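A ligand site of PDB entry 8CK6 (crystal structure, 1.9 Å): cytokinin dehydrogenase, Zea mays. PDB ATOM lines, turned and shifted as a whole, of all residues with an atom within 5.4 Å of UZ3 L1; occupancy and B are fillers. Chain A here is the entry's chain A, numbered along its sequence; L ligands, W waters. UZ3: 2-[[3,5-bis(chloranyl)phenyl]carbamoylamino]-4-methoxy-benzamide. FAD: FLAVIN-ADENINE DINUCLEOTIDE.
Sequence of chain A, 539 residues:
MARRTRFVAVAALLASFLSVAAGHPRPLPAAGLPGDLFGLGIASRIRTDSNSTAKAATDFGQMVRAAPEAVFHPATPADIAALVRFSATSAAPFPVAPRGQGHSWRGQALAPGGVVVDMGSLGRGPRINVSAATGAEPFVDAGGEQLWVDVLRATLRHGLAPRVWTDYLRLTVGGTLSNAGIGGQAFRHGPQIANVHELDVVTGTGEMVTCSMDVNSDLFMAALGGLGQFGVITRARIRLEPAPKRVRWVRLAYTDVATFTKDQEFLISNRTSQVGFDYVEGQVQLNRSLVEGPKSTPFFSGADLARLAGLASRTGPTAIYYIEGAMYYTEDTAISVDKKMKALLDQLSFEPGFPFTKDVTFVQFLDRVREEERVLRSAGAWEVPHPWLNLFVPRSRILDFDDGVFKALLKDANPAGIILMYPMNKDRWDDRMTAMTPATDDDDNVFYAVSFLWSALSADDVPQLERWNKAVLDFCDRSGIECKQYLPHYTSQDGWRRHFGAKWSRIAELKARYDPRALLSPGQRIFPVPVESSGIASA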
ATOM      1  N   PHE A  60       9.055  24.056 -12.497  1.00  0.00           N
ATOM      2  CA  PHE A  60       9.002  22.778 -11.787  1.00  0.00           C
ATOM      3  C   PHE A  60       9.419  22.873 -10.282  1.00  0.00           C
ATOM      4  O   PHE A  60       8.948  22.075  -9.462  1.00  0.00           O
ATOM      5  CB  PHE A  60       9.847  21.746 -12.549  1.00  0.00           C
ATOM      6  CG  PHE A  60       9.902  20.374 -11.947  1.00  0.00           C
ATOM      7  CD1 PHE A  60       8.832  19.494 -12.088  1.00  0.00           C
ATOM      8  CD2 PHE A  60      11.022  19.948 -11.248  1.00  0.00           C
ATOM      9  CE1 PHE A  60       8.894  18.209 -11.548  1.00  0.00           C
ATOM     10  CE2 PHE A  60      11.092  18.663 -10.720  1.00  0.00           C
ATOM     11  CZ  PHE A  60      10.022  17.797 -10.878  1.00  0.00           C
ATOM     12  N   TRP A 105      14.305  24.666 -11.736  1.00  0.00           N
ATOM     13  CA  TRP A 105      13.704  24.885 -10.418  1.00  0.00           C
ATOM     14  C   TRP A 105      14.203  26.140  -9.698  1.00  0.00           C
ATOM     15  O   TRP A 105      13.813  26.370  -8.550  1.00  0.00           O
ATOM     16  CB  TRP A 105      13.872  23.627  -9.514  1.00  0.00           C
ATOM     17  CG  TRP A 105      15.236  23.042  -9.529  1.00  0.00           C
ATOM     18  CD1 TRP A 105      16.258  23.301  -8.664  1.00  0.00           C
ATOM     19  CD2 TRP A 105      15.766  22.164 -10.527  1.00  0.00           C
ATOM     20  NE1 TRP A 105      17.399  22.637  -9.067  1.00  0.00           N
ATOM     21  CE2 TRP A 105      17.128  21.945 -10.218  1.00  0.00           C
ATOM     22  CE3 TRP A 105      15.204  21.526 -11.658  1.00  0.00           C
ATOM     23  CZ2 TRP A 105      17.927  21.092 -10.983  1.00  0.00           C
ATOM     24  CZ3 TRP A 105      16.013  20.716 -12.434  1.00  0.00           C
ATOM     25  CH2 TRP A 105      17.368  20.525 -12.112  1.00  0.00           C
ATOM     26  N   ASP A 167      17.130  11.056 -18.009  1.00  0.00           N
ATOM     27  CA  ASP A 167      16.212  10.104 -17.375  1.00  0.00           C
ATOM     28  C   ASP A 167      14.764  10.426 -17.687  1.00  0.00           C
ATOM     29  O   ASP A 167      13.903   9.571 -17.499  1.00  0.00           O
ATOM     30  CB  ASP A 167      16.359  10.167 -15.854  1.00  0.00           C
ATOM     31  CG  ASP A 167      17.732   9.744 -15.373  1.00  0.00           C
ATOM     32  OD1 ASP A 167      18.406   8.981 -16.099  1.00  0.00           O
ATOM     33  OD2 ASP A 167      18.112  10.164 -14.272  1.00  0.00           O
ATOM     34  N   ILE A 182      22.762  14.773 -19.251  1.00  0.00           N
ATOM     35  CA  ILE A 182      23.461  13.577 -18.782  1.00  0.00           C
ATOM     36  C   ILE A 182      22.450  12.455 -18.489  1.00  0.00           C
ATOM     37  O   ILE A 182      21.264  12.703 -18.299  1.00  0.00           O
ATOM     38  CB  ILE A 182      24.444  13.879 -17.601  1.00  0.00           C
ATOM     39  CG1 ILE A 182      23.686  14.197 -16.306  1.00  0.00           C
ATOM     40  CG2 ILE A 182      25.447  15.024 -17.974  1.00  0.00           C
ATOM     41  CD1 ILE A 182      24.594  14.343 -15.037  1.00  0.00           C
ATOM     42  N   ARG A 251      18.711  -3.855 -11.133  1.00  0.00           N
ATOM     43  CA  ARG A 251      19.097  -3.048  -9.986  1.00  0.00           C
ATOM     44  C   ARG A 251      19.792  -4.030  -9.070  1.00  0.00           C
ATOM     45  O   ARG A 251      19.272  -5.134  -8.847  1.00  0.00           O
ATOM     46  CB  ARG A 251      17.925  -2.362  -9.302  1.00  0.00           C
ATOM     47  CG  ARG A 251      17.563  -1.086 -10.061  1.00  0.00           C
ATOM     48  CD  ARG A 251      16.516  -0.272  -9.358  1.00  0.00           C
ATOM     49  NE  ARG A 251      15.968   0.753 -10.241  1.00  0.00           N
ATOM     50  CZ  ARG A 251      14.981   1.562  -9.900  1.00  0.00           C
ATOM     51  NH1 ARG A 251      14.541   2.475 -10.759  1.00  0.00           N
ATOM     52  NH2 ARG A 251      14.417   1.458  -8.711  1.00  0.00           N
ATOM     53  N   GLU A 281      23.725   3.623 -14.031  1.00  0.00           N
ATOM     54  CA  GLU A 281      23.392   4.656 -13.052  1.00  0.00           C
ATOM     55  C   GLU A 281      23.478   4.004 -11.671  1.00  0.00           C
ATOM     56  O   GLU A 281      23.897   2.843 -11.525  1.00  0.00           O
ATOM     57  CB  GLU A 281      22.017   5.285 -13.300  1.00  0.00           C
ATOM     58  CG  GLU A 281      22.000   6.199 -14.521  1.00  0.00           C
ATOM     59  CD  GLU A 281      20.830   7.148 -14.633  1.00  0.00           C
ATOM     60  OE1 GLU A 281      20.696   7.766 -15.711  1.00  0.00           O
ATOM     61  OE2 GLU A 281      20.049   7.286 -13.660  1.00  0.00           O
ATOM     62  N   GLN A 283      21.640   4.639  -7.360  1.00  0.00           N
ATOM     63  CA  GLN A 283      20.768   5.356  -6.433  1.00  0.00           C
ATOM     64  C   GLN A 283      21.180   5.107  -5.008  1.00  0.00           C
ATOM     65  O   GLN A 283      21.620   4.010  -4.681  1.00  0.00           O
ATOM     66  CB  GLN A 283      19.288   4.932  -6.610  1.00  0.00           C
ATOM     67  CG  GLN A 283      18.710   5.335  -7.979  1.00  0.00           C
ATOM     68  CD  GLN A 283      17.296   4.868  -8.231  1.00  0.00           C
ATOM     69  OE1 GLN A 283      16.592   4.368  -7.347  1.00  0.00           O
ATOM     70  NE2 GLN A 283      16.877   5.027  -9.462  1.00  0.00           N
ATOM     71  N   ARG A 368      10.764   5.083 -18.784  1.00  0.00           N
ATOM     72  CA  ARG A 368      10.516   4.530 -17.443  1.00  0.00           C
ATOM     73  C   ARG A 368      10.039   5.553 -16.403  1.00  0.00           C
ATOM     74  O   ARG A 368       9.207   5.215 -15.564  1.00  0.00           O
ATOM     75  CB  ARG A 368      11.748   3.757 -16.901  1.00  0.00           C
ATOM     76  CG  ARG A 368      12.979   4.624 -16.544  1.00  0.00           C
ATOM     77  CD  ARG A 368      14.317   3.882 -16.494  1.00  0.00           C
ATOM     78  NE  ARG A 368      15.409   4.836 -16.247  1.00  0.00           N
ATOM     79  CZ  ARG A 368      15.957   5.613 -17.177  1.00  0.00           C
ATOM     80  NH1 ARG A 368      15.611   5.494 -18.455  1.00  0.00           N
ATOM     81  NH2 ARG A 368      16.861   6.523 -16.839  1.00  0.00           N
ATOM     82  N   VAL A 369      10.584   6.792 -16.444  1.00  0.00           N
ATOM     83  CA  VAL A 369      10.260   7.810 -15.443  1.00  0.00           C
ATOM     84  C   VAL A 369       8.830   8.334 -15.651  1.00  0.00           C
ATOM     85  O   VAL A 369       8.204   8.784 -14.690  1.00  0.00           O
ATOM     86  CB  VAL A 369      11.354   8.931 -15.336  1.00  0.00           C
ATOM     87  CG1 VAL A 369      10.962  10.044 -14.369  1.00  0.00           C
ATOM     88  CG2 VAL A 369      12.686   8.320 -14.922  1.00  0.00           C
ATOM     89  N   GLU A 372       6.748   6.537 -13.288  1.00  0.00           N
ATOM     90  CA  GLU A 372       6.979   7.033 -11.938  1.00  0.00           C
ATOM     91  C   GLU A 372       6.212   8.339 -11.717  1.00  0.00           C
ATOM     92  O   GLU A 372       5.597   8.532 -10.666  1.00  0.00           O
ATOM     93  CB  GLU A 372       8.493   7.191 -11.650  1.00  0.00           C
ATOM     94  CG  GLU A 372       9.233   5.877 -11.830  1.00  0.00           C
ATOM     95  CD  GLU A 372      10.701   5.944 -11.513  1.00  0.00           C
ATOM     96  OE1 GLU A 372      11.063   5.767 -10.325  1.00  0.00           O
ATOM     97  OE2 GLU A 372      11.499   6.172 -12.440  1.00  0.00           O
ATOM     98  N   LEU A 376       3.359   9.280  -8.954  1.00  0.00           N
ATOM     99  CA  LEU A 376       3.519  10.475  -8.127  1.00  0.00           C
ATOM    100  C   LEU A 376       2.382  11.451  -8.252  1.00  0.00           C
ATOM    101  O   LEU A 376       1.959  11.991  -7.231  1.00  0.00           O
ATOM    102  CB  LEU A 376       4.860  11.171  -8.385  1.00  0.00           C
ATOM    103  CG  LEU A 376       6.098  10.399  -7.872  1.00  0.00           C
ATOM    104  CD1 LEU A 376       7.362  10.885  -8.576  1.00  0.00           C
ATOM    105  CD2 LEU A 376       6.251  10.497  -6.339  1.00  0.00           C
ATOM    106  N   TRP A 382       3.806  15.122  -7.183  1.00  0.00           N
ATOM    107  CA  TRP A 382       4.602  15.563  -8.335  1.00  0.00           C
ATOM    108  C   TRP A 382       4.623  17.093  -8.415  1.00  0.00           C
ATOM    109  O   TRP A 382       5.698  17.669  -8.521  1.00  0.00           O
ATOM    110  CB  TRP A 382       4.094  14.942  -9.648  1.00  0.00           C
ATOM    111  CG  TRP A 382       4.893  15.355 -10.865  1.00  0.00           C
ATOM    112  CD1 TRP A 382       4.648  16.402 -11.702  1.00  0.00           C
ATOM    113  CD2 TRP A 382       6.069  14.706 -11.363  1.00  0.00           C
ATOM    114  NE1 TRP A 382       5.590  16.442 -12.691  1.00  0.00           N
ATOM    115  CE2 TRP A 382       6.474  15.403 -12.523  1.00  0.00           C
ATOM    116  CE3 TRP A 382       6.783  13.569 -10.968  1.00  0.00           C
ATOM    117  CZ2 TRP A 382       7.578  15.006 -13.281  1.00  0.00           C
ATOM    118  CZ3 TRP A 382       7.884  13.178 -11.719  1.00  0.00           C
ATOM    119  CH2 TRP A 382       8.260  13.883 -12.872  1.00  0.00           C
ATOM    120  N   HIS A 386      10.513  21.460  -5.555  1.00  0.00           N
ATOM    121  CA  HIS A 386      11.678  20.622  -5.844  1.00  0.00           C
ATOM    122  C   HIS A 386      12.954  21.435  -5.643  1.00  0.00           C
ATOM    123  O   HIS A 386      13.526  21.936  -6.617  1.00  0.00           O
ATOM    124  CB  HIS A 386      11.624  20.028  -7.260  1.00  0.00           C
ATOM    125  CG  HIS A 386      10.439  19.161  -7.481  1.00  0.00           C
ATOM    126  ND1 HIS A 386       9.311  19.636  -8.126  1.00  0.00           N
ATOM    127  CD2 HIS A 386      10.238  17.871  -7.145  1.00  0.00           C
ATOM    128  CE1 HIS A 386       8.460  18.624  -8.157  1.00  0.00           C
ATOM    129  NE2 HIS A 386       8.970  17.538  -7.581  1.00  0.00           N
ATOM    130  N   TRP A 388      16.058  21.070  -5.672  1.00  0.00           N
ATOM    131  CA  TRP A 388      17.051  20.117  -6.150  1.00  0.00           C
ATOM    132  C   TRP A 388      18.465  20.648  -6.180  1.00  0.00           C
ATOM    133  O   TRP A 388      18.671  21.855  -6.323  1.00  0.00           O
ATOM    134  CB  TRP A 388      16.638  19.600  -7.530  1.00  0.00           C
ATOM    135  CG  TRP A 388      15.460  18.678  -7.539  1.00  0.00           C
ATOM    136  CD1 TRP A 388      14.721  18.258  -6.459  1.00  0.00           C
ATOM    137  CD2 TRP A 388      14.935  17.967  -8.681  1.00  0.00           C
ATOM    138  NE1 TRP A 388      13.793  17.330  -6.854  1.00  0.00           N
ATOM    139  CE2 TRP A 388      13.909  17.117  -8.204  1.00  0.00           C
ATOM    140  CE3 TRP A 388      15.230  17.988 -10.052  1.00  0.00           C
ATOM    141  CZ2 TRP A 388      13.156  16.301  -9.063  1.00  0.00           C
ATOM    142  CZ3 TRP A 388      14.511  17.142 -10.891  1.00  0.00           C
ATOM    143  CH2 TRP A 388      13.490  16.313 -10.403  1.00  0.00           C
ATOM    144  N   ASN A 390      22.444  19.324  -7.792  1.00  0.00           N
ATOM    145  CA  ASN A 390      23.190  18.384  -8.631  1.00  0.00           C
ATOM    146  C   ASN A 390      24.657  18.748  -8.571  1.00  0.00           C
ATOM    147  O   ASN A 390      25.007  19.916  -8.799  1.00  0.00           O
ATOM    148  CB  ASN A 390      22.651  18.419 -10.061  1.00  0.00           C
ATOM    149  CG  ASN A 390      21.177  18.112 -10.142  1.00  0.00           C
ATOM    150  OD1 ASN A 390      20.763  16.967 -10.361  1.00  0.00           O
ATOM    151  ND2 ASN A 390      20.338  19.102  -9.909  1.00  0.00           N
ATOM    152  N   ILE A 418      14.348  11.121  -4.699  1.00  0.00           N
ATOM    153  CA  ILE A 418      15.386  10.175  -5.001  1.00  0.00           C
ATOM    154  C   ILE A 418      16.747  10.833  -4.913  1.00  0.00           C
ATOM    155  O   ILE A 418      16.839  12.063  -4.985  1.00  0.00           O
ATOM    156  CB  ILE A 418      15.054   9.607  -6.422  1.00  0.00           C
ATOM    157  CG1 ILE A 418      15.696   8.229  -6.696  1.00  0.00           C
ATOM    158  CG2 ILE A 418      15.356  10.576  -7.544  1.00  0.00           C
ATOM    159  CD1 ILE A 418      14.992   7.478  -7.874  1.00  0.00           C
ATOM    160  N   LEU A 420      20.463  10.193  -6.817  1.00  0.00           N
ATOM    161  CA  LEU A 420      21.239   9.498  -7.853  1.00  0.00           C
ATOM    162  C   LEU A 420      22.724   9.665  -7.592  1.00  0.00           C
ATOM    163  O   LEU A 420      23.171  10.723  -7.112  1.00  0.00           O
ATOM    164  CB  LEU A 420      20.938   9.991  -9.301  1.00  0.00           C
ATOM    165  CG  LEU A 420      19.482  10.014  -9.760  1.00  0.00           C
ATOM    166  CD1 LEU A 420      19.408  10.504 -11.176  1.00  0.00           C
ATOM    167  CD2 LEU A 420      18.816   8.649  -9.612  1.00  0.00           C
ATOM    168  N   TYR A 422      26.293   8.218  -9.773  1.00  0.00           N
ATOM    169  CA  TYR A 422      26.951   7.370 -10.766  1.00  0.00           C
ATOM    170  C   TYR A 422      28.169   8.061 -11.358  1.00  0.00           C
ATOM    171  O   TYR A 422      28.171   9.289 -11.493  1.00  0.00           O
ATOM    172  CB  TYR A 422      25.984   6.896 -11.873  1.00  0.00           C
ATOM    173  CG  TYR A 422      25.310   7.981 -12.700  1.00  0.00           C
ATOM    174  CD1 TYR A 422      24.058   8.474 -12.342  1.00  0.00           C
ATOM    175  CD2 TYR A 422      25.857   8.405 -13.907  1.00  0.00           C
ATOM    176  CE1 TYR A 422      23.390   9.416 -13.133  1.00  0.00           C
ATOM    177  CE2 TYR A 422      25.214   9.374 -14.699  1.00  0.00           C
ATOM    178  CZ  TYR A 422      23.982   9.879 -14.295  1.00  0.00           C
ATOM    179  OH  TYR A 422      23.330  10.806 -15.077  1.00  0.00           O
ATOM    180  N   ALA A 449      28.416  11.945 -10.649  1.00  0.00           N
ATOM    181  CA  ALA A 449      27.290  12.868 -10.626  1.00  0.00           C
ATOM    182  C   ALA A 449      26.485  12.419  -9.421  1.00  0.00           C
ATOM    183  O   ALA A 449      26.189  11.217  -9.285  1.00  0.00           O
ATOM    184  CB  ALA A 449      26.457  12.761 -11.897  1.00  0.00           C
ATOM    185  N   SER A 451      23.015  13.570  -7.429  1.00  0.00           N
ATOM    186  CA  SER A 451      21.814  14.409  -7.578  1.00  0.00           C
ATOM    187  C   SER A 451      20.889  14.214  -6.405  1.00  0.00           C
ATOM    188  O   SER A 451      20.423  13.100  -6.174  1.00  0.00           O
ATOM    189  CB  SER A 451      21.097  14.079  -8.887  1.00  0.00           C
ATOM    190  OG  SER A 451      21.935  14.291 -10.014  1.00  0.00           O
ATOM    191  N   LEU A 453      17.507  14.857  -5.574  1.00  0.00           N
ATOM    192  CA  LEU A 453      16.224  15.140  -6.233  1.00  0.00           C
ATOM    193  C   LEU A 453      15.125  14.977  -5.192  1.00  0.00           C
ATOM    194  O   LEU A 453      14.224  14.154  -5.337  1.00  0.00           O
ATOM    195  CB  LEU A 453      16.028  14.169  -7.397  1.00  0.00           C
ATOM    196  CG  LEU A 453      17.216  14.122  -8.392  1.00  0.00           C
ATOM    197  CD1 LEU A 453      16.955  13.116  -9.455  1.00  0.00           C
ATOM    198  CD2 LEU A 453      17.523  15.522  -8.986  1.00  0.00           C
ATOM    199  N   TYR A 486      26.091  20.928 -11.259  1.00  0.00           N
ATOM    200  CA  TYR A 486      25.518  20.628 -12.570  1.00  0.00           C
ATOM    201  C   TYR A 486      24.141  21.304 -12.487  1.00  0.00           C
ATOM    202  O   TYR A 486      23.603  21.371 -11.381  1.00  0.00           O
ATOM    203  CB  TYR A 486      25.412  19.133 -12.882  1.00  0.00           C
ATOM    204  CG  TYR A 486      24.689  18.860 -14.195  1.00  0.00           C
ATOM    205  CD1 TYR A 486      25.105  19.473 -15.382  1.00  0.00           C
ATOM    206  CD2 TYR A 486      23.616  17.978 -14.255  1.00  0.00           C
ATOM    207  CE1 TYR A 486      24.390  19.302 -16.564  1.00  0.00           C
ATOM    208  CE2 TYR A 486      22.934  17.757 -15.459  1.00  0.00           C
ATOM    209  CZ  TYR A 486      23.321  18.426 -16.613  1.00  0.00           C
ATOM    210  OH  TYR A 486      22.617  18.283 -17.772  1.00  0.00           O
ATOM    211  N   LEU A 487      23.623  21.873 -13.595  1.00  0.00           N
ATOM    212  CA  LEU A 487      22.365  22.681 -13.579  1.00  0.00           C
ATOM    213  C   LEU A 487      22.581  23.774 -12.510  1.00  0.00           C
ATOM    214  O   LEU A 487      21.822  23.855 -11.541  1.00  0.00           O
ATOM    215  CB  LEU A 487      21.125  21.781 -13.293  1.00  0.00           C
ATOM    216  CG  LEU A 487      21.010  20.610 -14.267  1.00  0.00           C
ATOM    217  CD1 LEU A 487      20.286  19.426 -13.663  1.00  0.00           C
ATOM    218  CD2 LEU A 487      20.421  21.054 -15.576  1.00  0.00           C
HETATM  219  CAJ UZ3 L   1      17.223  14.820 -12.699  1.00  0.00           C
HETATM  220  CAR UZ3 L   1      18.157  15.847 -12.783  1.00  0.00           C
HETATM  221 CLAE UZ3 L   1      17.666  17.486 -12.481  1.00  0.00          CL
HETATM  222  CAI UZ3 L   1      19.490  15.617 -13.057  1.00  0.00           C
HETATM  223  CAS UZ3 L   1      19.880  14.313 -13.296  1.00  0.00           C
HETATM  224 CLAF UZ3 L   1      21.566  13.951 -13.660  1.00  0.00          CL
HETATM  225  CAK UZ3 L   1      18.976  13.271 -13.226  1.00  0.00           C
HETATM  226  CAT UZ3 L   1      17.638  13.546 -13.055  1.00  0.00           C
HETATM  227  NAM UZ3 L   1      16.808  12.387 -12.924  1.00  0.00           N
HETATM  228  CAQ UZ3 L   1      15.473  12.397 -12.419  1.00  0.00           C
HETATM  229  OAD UZ3 L   1      14.851  13.385 -12.176  1.00  0.00           O
HETATM  230  NAN UZ3 L   1      14.982  11.067 -12.246  1.00  0.00           N
HETATM  231  CAV UZ3 L   1      13.708  10.663 -11.688  1.00  0.00           C
HETATM  232  CAL UZ3 L   1      12.835  11.618 -11.176  1.00  0.00           C
HETATM  233  CAU UZ3 L   1      11.680  11.227 -10.504  1.00  0.00           C
HETATM  234  OAO UZ3 L   1      10.701  12.147 -10.091  1.00  0.00           O
HETATM  235  CAA UZ3 L   1      11.045  13.509  -9.947  1.00  0.00           C
HETATM  236  CAG UZ3 L   1      11.447   9.865 -10.312  1.00  0.00           C
HETATM  237  CAH UZ3 L   1      12.379   8.912 -10.730  1.00  0.00           C
HETATM  238  CAW UZ3 L   1      13.546   9.315 -11.362  1.00  0.00           C
HETATM  239  CAP UZ3 L   1      14.578   8.260 -11.817  1.00  0.00           C
HETATM  240  OAC UZ3 L   1      15.615   8.572 -12.305  1.00  0.00           O
HETATM  241  NAB UZ3 L   1      14.313   6.850 -11.654  1.00  0.00           N
HETATM  242  PA  FAD L   2      13.385  25.147 -19.251  1.00  0.00           P
HETATM  243  O1A FAD L   2      13.204  24.605 -17.885  1.00  0.00           O
HETATM  244  O2A FAD L   2      12.093  25.731 -19.790  1.00  0.00           O
HETATM  245  O5B FAD L   2      14.575  26.215 -19.401  1.00  0.00           O
HETATM  246  C5B FAD L   2      15.864  25.996 -18.763  1.00  0.00           C
HETATM  247  C4B FAD L   2      16.833  27.081 -19.182  1.00  0.00           C
HETATM  248  O4B FAD L   2      17.210  26.914 -20.571  1.00  0.00           O
HETATM  249  C3B FAD L   2      16.314  28.514 -19.065  1.00  0.00           C
HETATM  250  O3B FAD L   2      17.389  29.397 -18.779  1.00  0.00           O
HETATM  251  C2B FAD L   2      15.712  28.748 -20.450  1.00  0.00           C
HETATM  252  O2B FAD L   2      15.513  30.132 -20.759  1.00  0.00           O
HETATM  253  C1B FAD L   2      16.746  28.017 -21.335  1.00  0.00           C
HETATM  254  N9A FAD L   2      16.233  27.501 -22.610  1.00  0.00           N
HETATM  255  C8A FAD L   2      15.129  26.724 -22.822  1.00  0.00           C
HETATM  256  N7A FAD L   2      14.987  26.341 -24.075  1.00  0.00           N
HETATM  257  C5A FAD L   2      16.061  26.933 -24.730  1.00  0.00           C
HETATM  258  C6A FAD L   2      16.472  26.934 -26.081  1.00  0.00           C
HETATM  259  N6A FAD L   2      15.786  26.346 -27.064  1.00  0.00           N
HETATM  260  N1A FAD L   2      17.608  27.605 -26.390  1.00  0.00           N
HETATM  261  C2A FAD L   2      18.279  28.223 -25.416  1.00  0.00           C
HETATM  262  N3A FAD L   2      17.983  28.303 -24.111  1.00  0.00           N
HETATM  263  C4A FAD L   2      16.850  27.639 -23.824  1.00  0.00           C
HETATM  264  N1  FAD L   2      18.981  16.823 -16.825  1.00  0.00           N
HETATM  265  C2  FAD L   2      19.898  15.933 -17.193  1.00  0.00           C
HETATM  266  O2  FAD L   2      20.917  16.285 -17.800  1.00  0.00           O
HETATM  267  N3  FAD L   2      19.695  14.590 -16.991  1.00  0.00           N
HETATM  268  C4  FAD L   2      18.525  14.014 -16.503  1.00  0.00           C
HETATM  269  O4  FAD L   2      18.462  12.795 -16.364  1.00  0.00           O
HETATM  270  C4X FAD L   2      17.496  14.974 -16.195  1.00  0.00           C
HETATM  271  N5  FAD L   2      16.329  14.521 -15.796  1.00  0.00           N
HETATM  272  C5X FAD L   2      15.378  15.461 -15.407  1.00  0.00           C
HETATM  273  C6  FAD L   2      14.166  15.013 -14.878  1.00  0.00           C
HETATM  274  C7  FAD L   2      13.179  15.905 -14.454  1.00  0.00           C
HETATM  275  C7M FAD L   2      11.884  15.360 -13.893  1.00  0.00           C
HETATM  276  C8  FAD L   2      13.405  17.287 -14.575  1.00  0.00           C
HETATM  277  C8M FAD L   2      12.352  18.301 -14.165  1.00  0.00           C
HETATM  278  C9  FAD L   2      14.615  17.741 -15.080  1.00  0.00           C
HETATM  279  C9A FAD L   2      15.611  16.849 -15.482  1.00  0.00           C
HETATM  280  N10 FAD L   2      16.875  17.279 -15.963  1.00  0.00           N
HETATM  281  C10 FAD L   2      17.828  16.381 -16.334  1.00  0.00           C
HETATM  282  C1' FAD L   2      17.210  18.713 -16.066  1.00  0.00           C
HETATM  283  C2' FAD L   2      16.898  19.324 -17.428  1.00  0.00           C
HETATM  284  O2' FAD L   2      17.718  18.733 -18.429  1.00  0.00           O
HETATM  285  C3' FAD L   2      17.196  20.821 -17.446  1.00  0.00           C
HETATM  286  O3' FAD L   2      16.561  21.451 -16.339  1.00  0.00           O
HETATM  287  C4' FAD L   2      16.928  21.550 -18.772  1.00  0.00           C
HETATM  288  O4' FAD L   2      16.877  22.954 -18.557  1.00  0.00           O
HETATM  289  C5' FAD L   2      15.730  21.055 -19.564  1.00  0.00           C
HETATM  290  O5' FAD L   2      14.588  21.849 -19.261  1.00  0.00           O
HETATM  291  P   FAD L   2      13.427  22.429 -20.317  1.00  0.00           P
HETATM  292  O1P FAD L   2      13.157  22.106 -21.740  1.00  0.00           O
HETATM  293  O2P FAD L   2      12.181  22.193 -19.467  1.00  0.00           O
HETATM  294  O3P FAD L   2      13.807  23.976 -20.234  1.00  0.00           O
HETATM  295  O   HOH W   1      17.152   7.037 -13.756  1.00  0.00           O
HETATM  296  O   HOH W   2      20.643  11.095 -15.215  1.00  0.00           O
HETATM  297  O   HOH W   3      13.433   4.825  -9.430  1.00  0.00           O
HETATM  298  O   HOH W   4      15.809   4.781 -13.166  1.00  0.00           O
HETATM  299  O   HOH W   5      13.027   4.040 -13.076  1.00  0.00           O
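O of Leu 420 is in hydrogen-bond range of N of Ser 451. The backbone carbonyl oxygen of Trp 388 is in hydrogen-bond range of the indole nitrogen of Trp 105, 3.1 Å away. The backbone NH of Leu 453 is in hydrogen-bond range of the backbone carbonyl oxygen of Ile 418 (2.9 Å). O of Trp 382 lies close to NE2 of His 386, 3.4 Å away. The side-chain carboxylate of Asp 167 lies within salt-bridge range of the guanidinium group of Arg 368 (3.0 Å). OD1 of Asp 167 sits close to OE1 of Glu 281 (2.6 Å). The backbone carbonyl oxygen (O) of Tyr 422 lies within hydrogen-bond range of the backbone NH (N) of Ala 449 (2.8 Å). The backbone NH of Tyr 486 is in hydrogen-bond range of the backbone carbonyl oxygen of Asn 390, at 2.9 Å.
O2 of FAD L2 is in hydrogen-bond range of N of Ile 182. A nitrogen (NAB) of UZ3 L1 is in hydrogen-bond range of the side-chain carboxylate (OE2) of Glu 372 (3.0 Å). An oxygen (O2) of FAD L2 is in hydrogen-bond range of the side-chain hydroxyl of Tyr 486 (2.6 Å). The backbone NH of Asp 167 sits at hydrogen-bond distance from an oxygen (O4) of FAD L2. A nitrogen (N3) of FAD L2 sits at hydrogen-bond distance from the backbone carbonyl oxygen (O) of Ile 182 (2.8 Å). The side-chain carboxylate (OD2) of Asp 167 sits at hydrogen-bond distance from a nitrogen (NAM) of UZ3 L1, 2.9 Å away.
Water W4 bridges NAB of UZ3 L1 (3.0 Å) and NE of Arg 368 (3.1 Å). Water W5 lies within hydrogen-bond range of OE2 of Glu 372 (2.7 Å), NH1 of Arg 251 (3.2 Å) and NAB of UZ3 L1 (3.4 Å).
CH2 of Trp 105 touches CLAE of UZ3 L1, at 3.1 Å. CD1 of Ile 182 touches CLAF of UZ3 L1, at 3.3 Å. NE2 of Gln 283 touches NAB of UZ3 L1 (3.8 Å). Val 369 touches UZ3 L1 (CG2 to CAP, 3.6 Å). Leu 376 touches UZ3 L1. Trp 382 touches UZ3 L1. Trp 388 touches UZ3 L1 (CE3 to CLAE, 3.5 Å). OD1 of Asn 390 touches CAI of UZ3 L1 (3.3 Å). Ile 418 touches UZ3 L1 (CD1 to NAB, 3.9 Å). Leu 420 touches UZ3 L1. OH of Tyr 422 touches CLAF of UZ3 L1, at 3.9 Å. Ser 451 touches UZ3 L1. CD1 of Leu 453 touches CAQ of UZ3 L1, at 3.4 Å. Leu 487 touches UZ3 L1 (CD1 to CLAE, 3.5 Å). Of the 23 residues printed, 16 come within 4 Å of UZ3 L1. The nearest printed residue that does not touch UZ3 L1 is Tyr 486 (4.4 Å).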
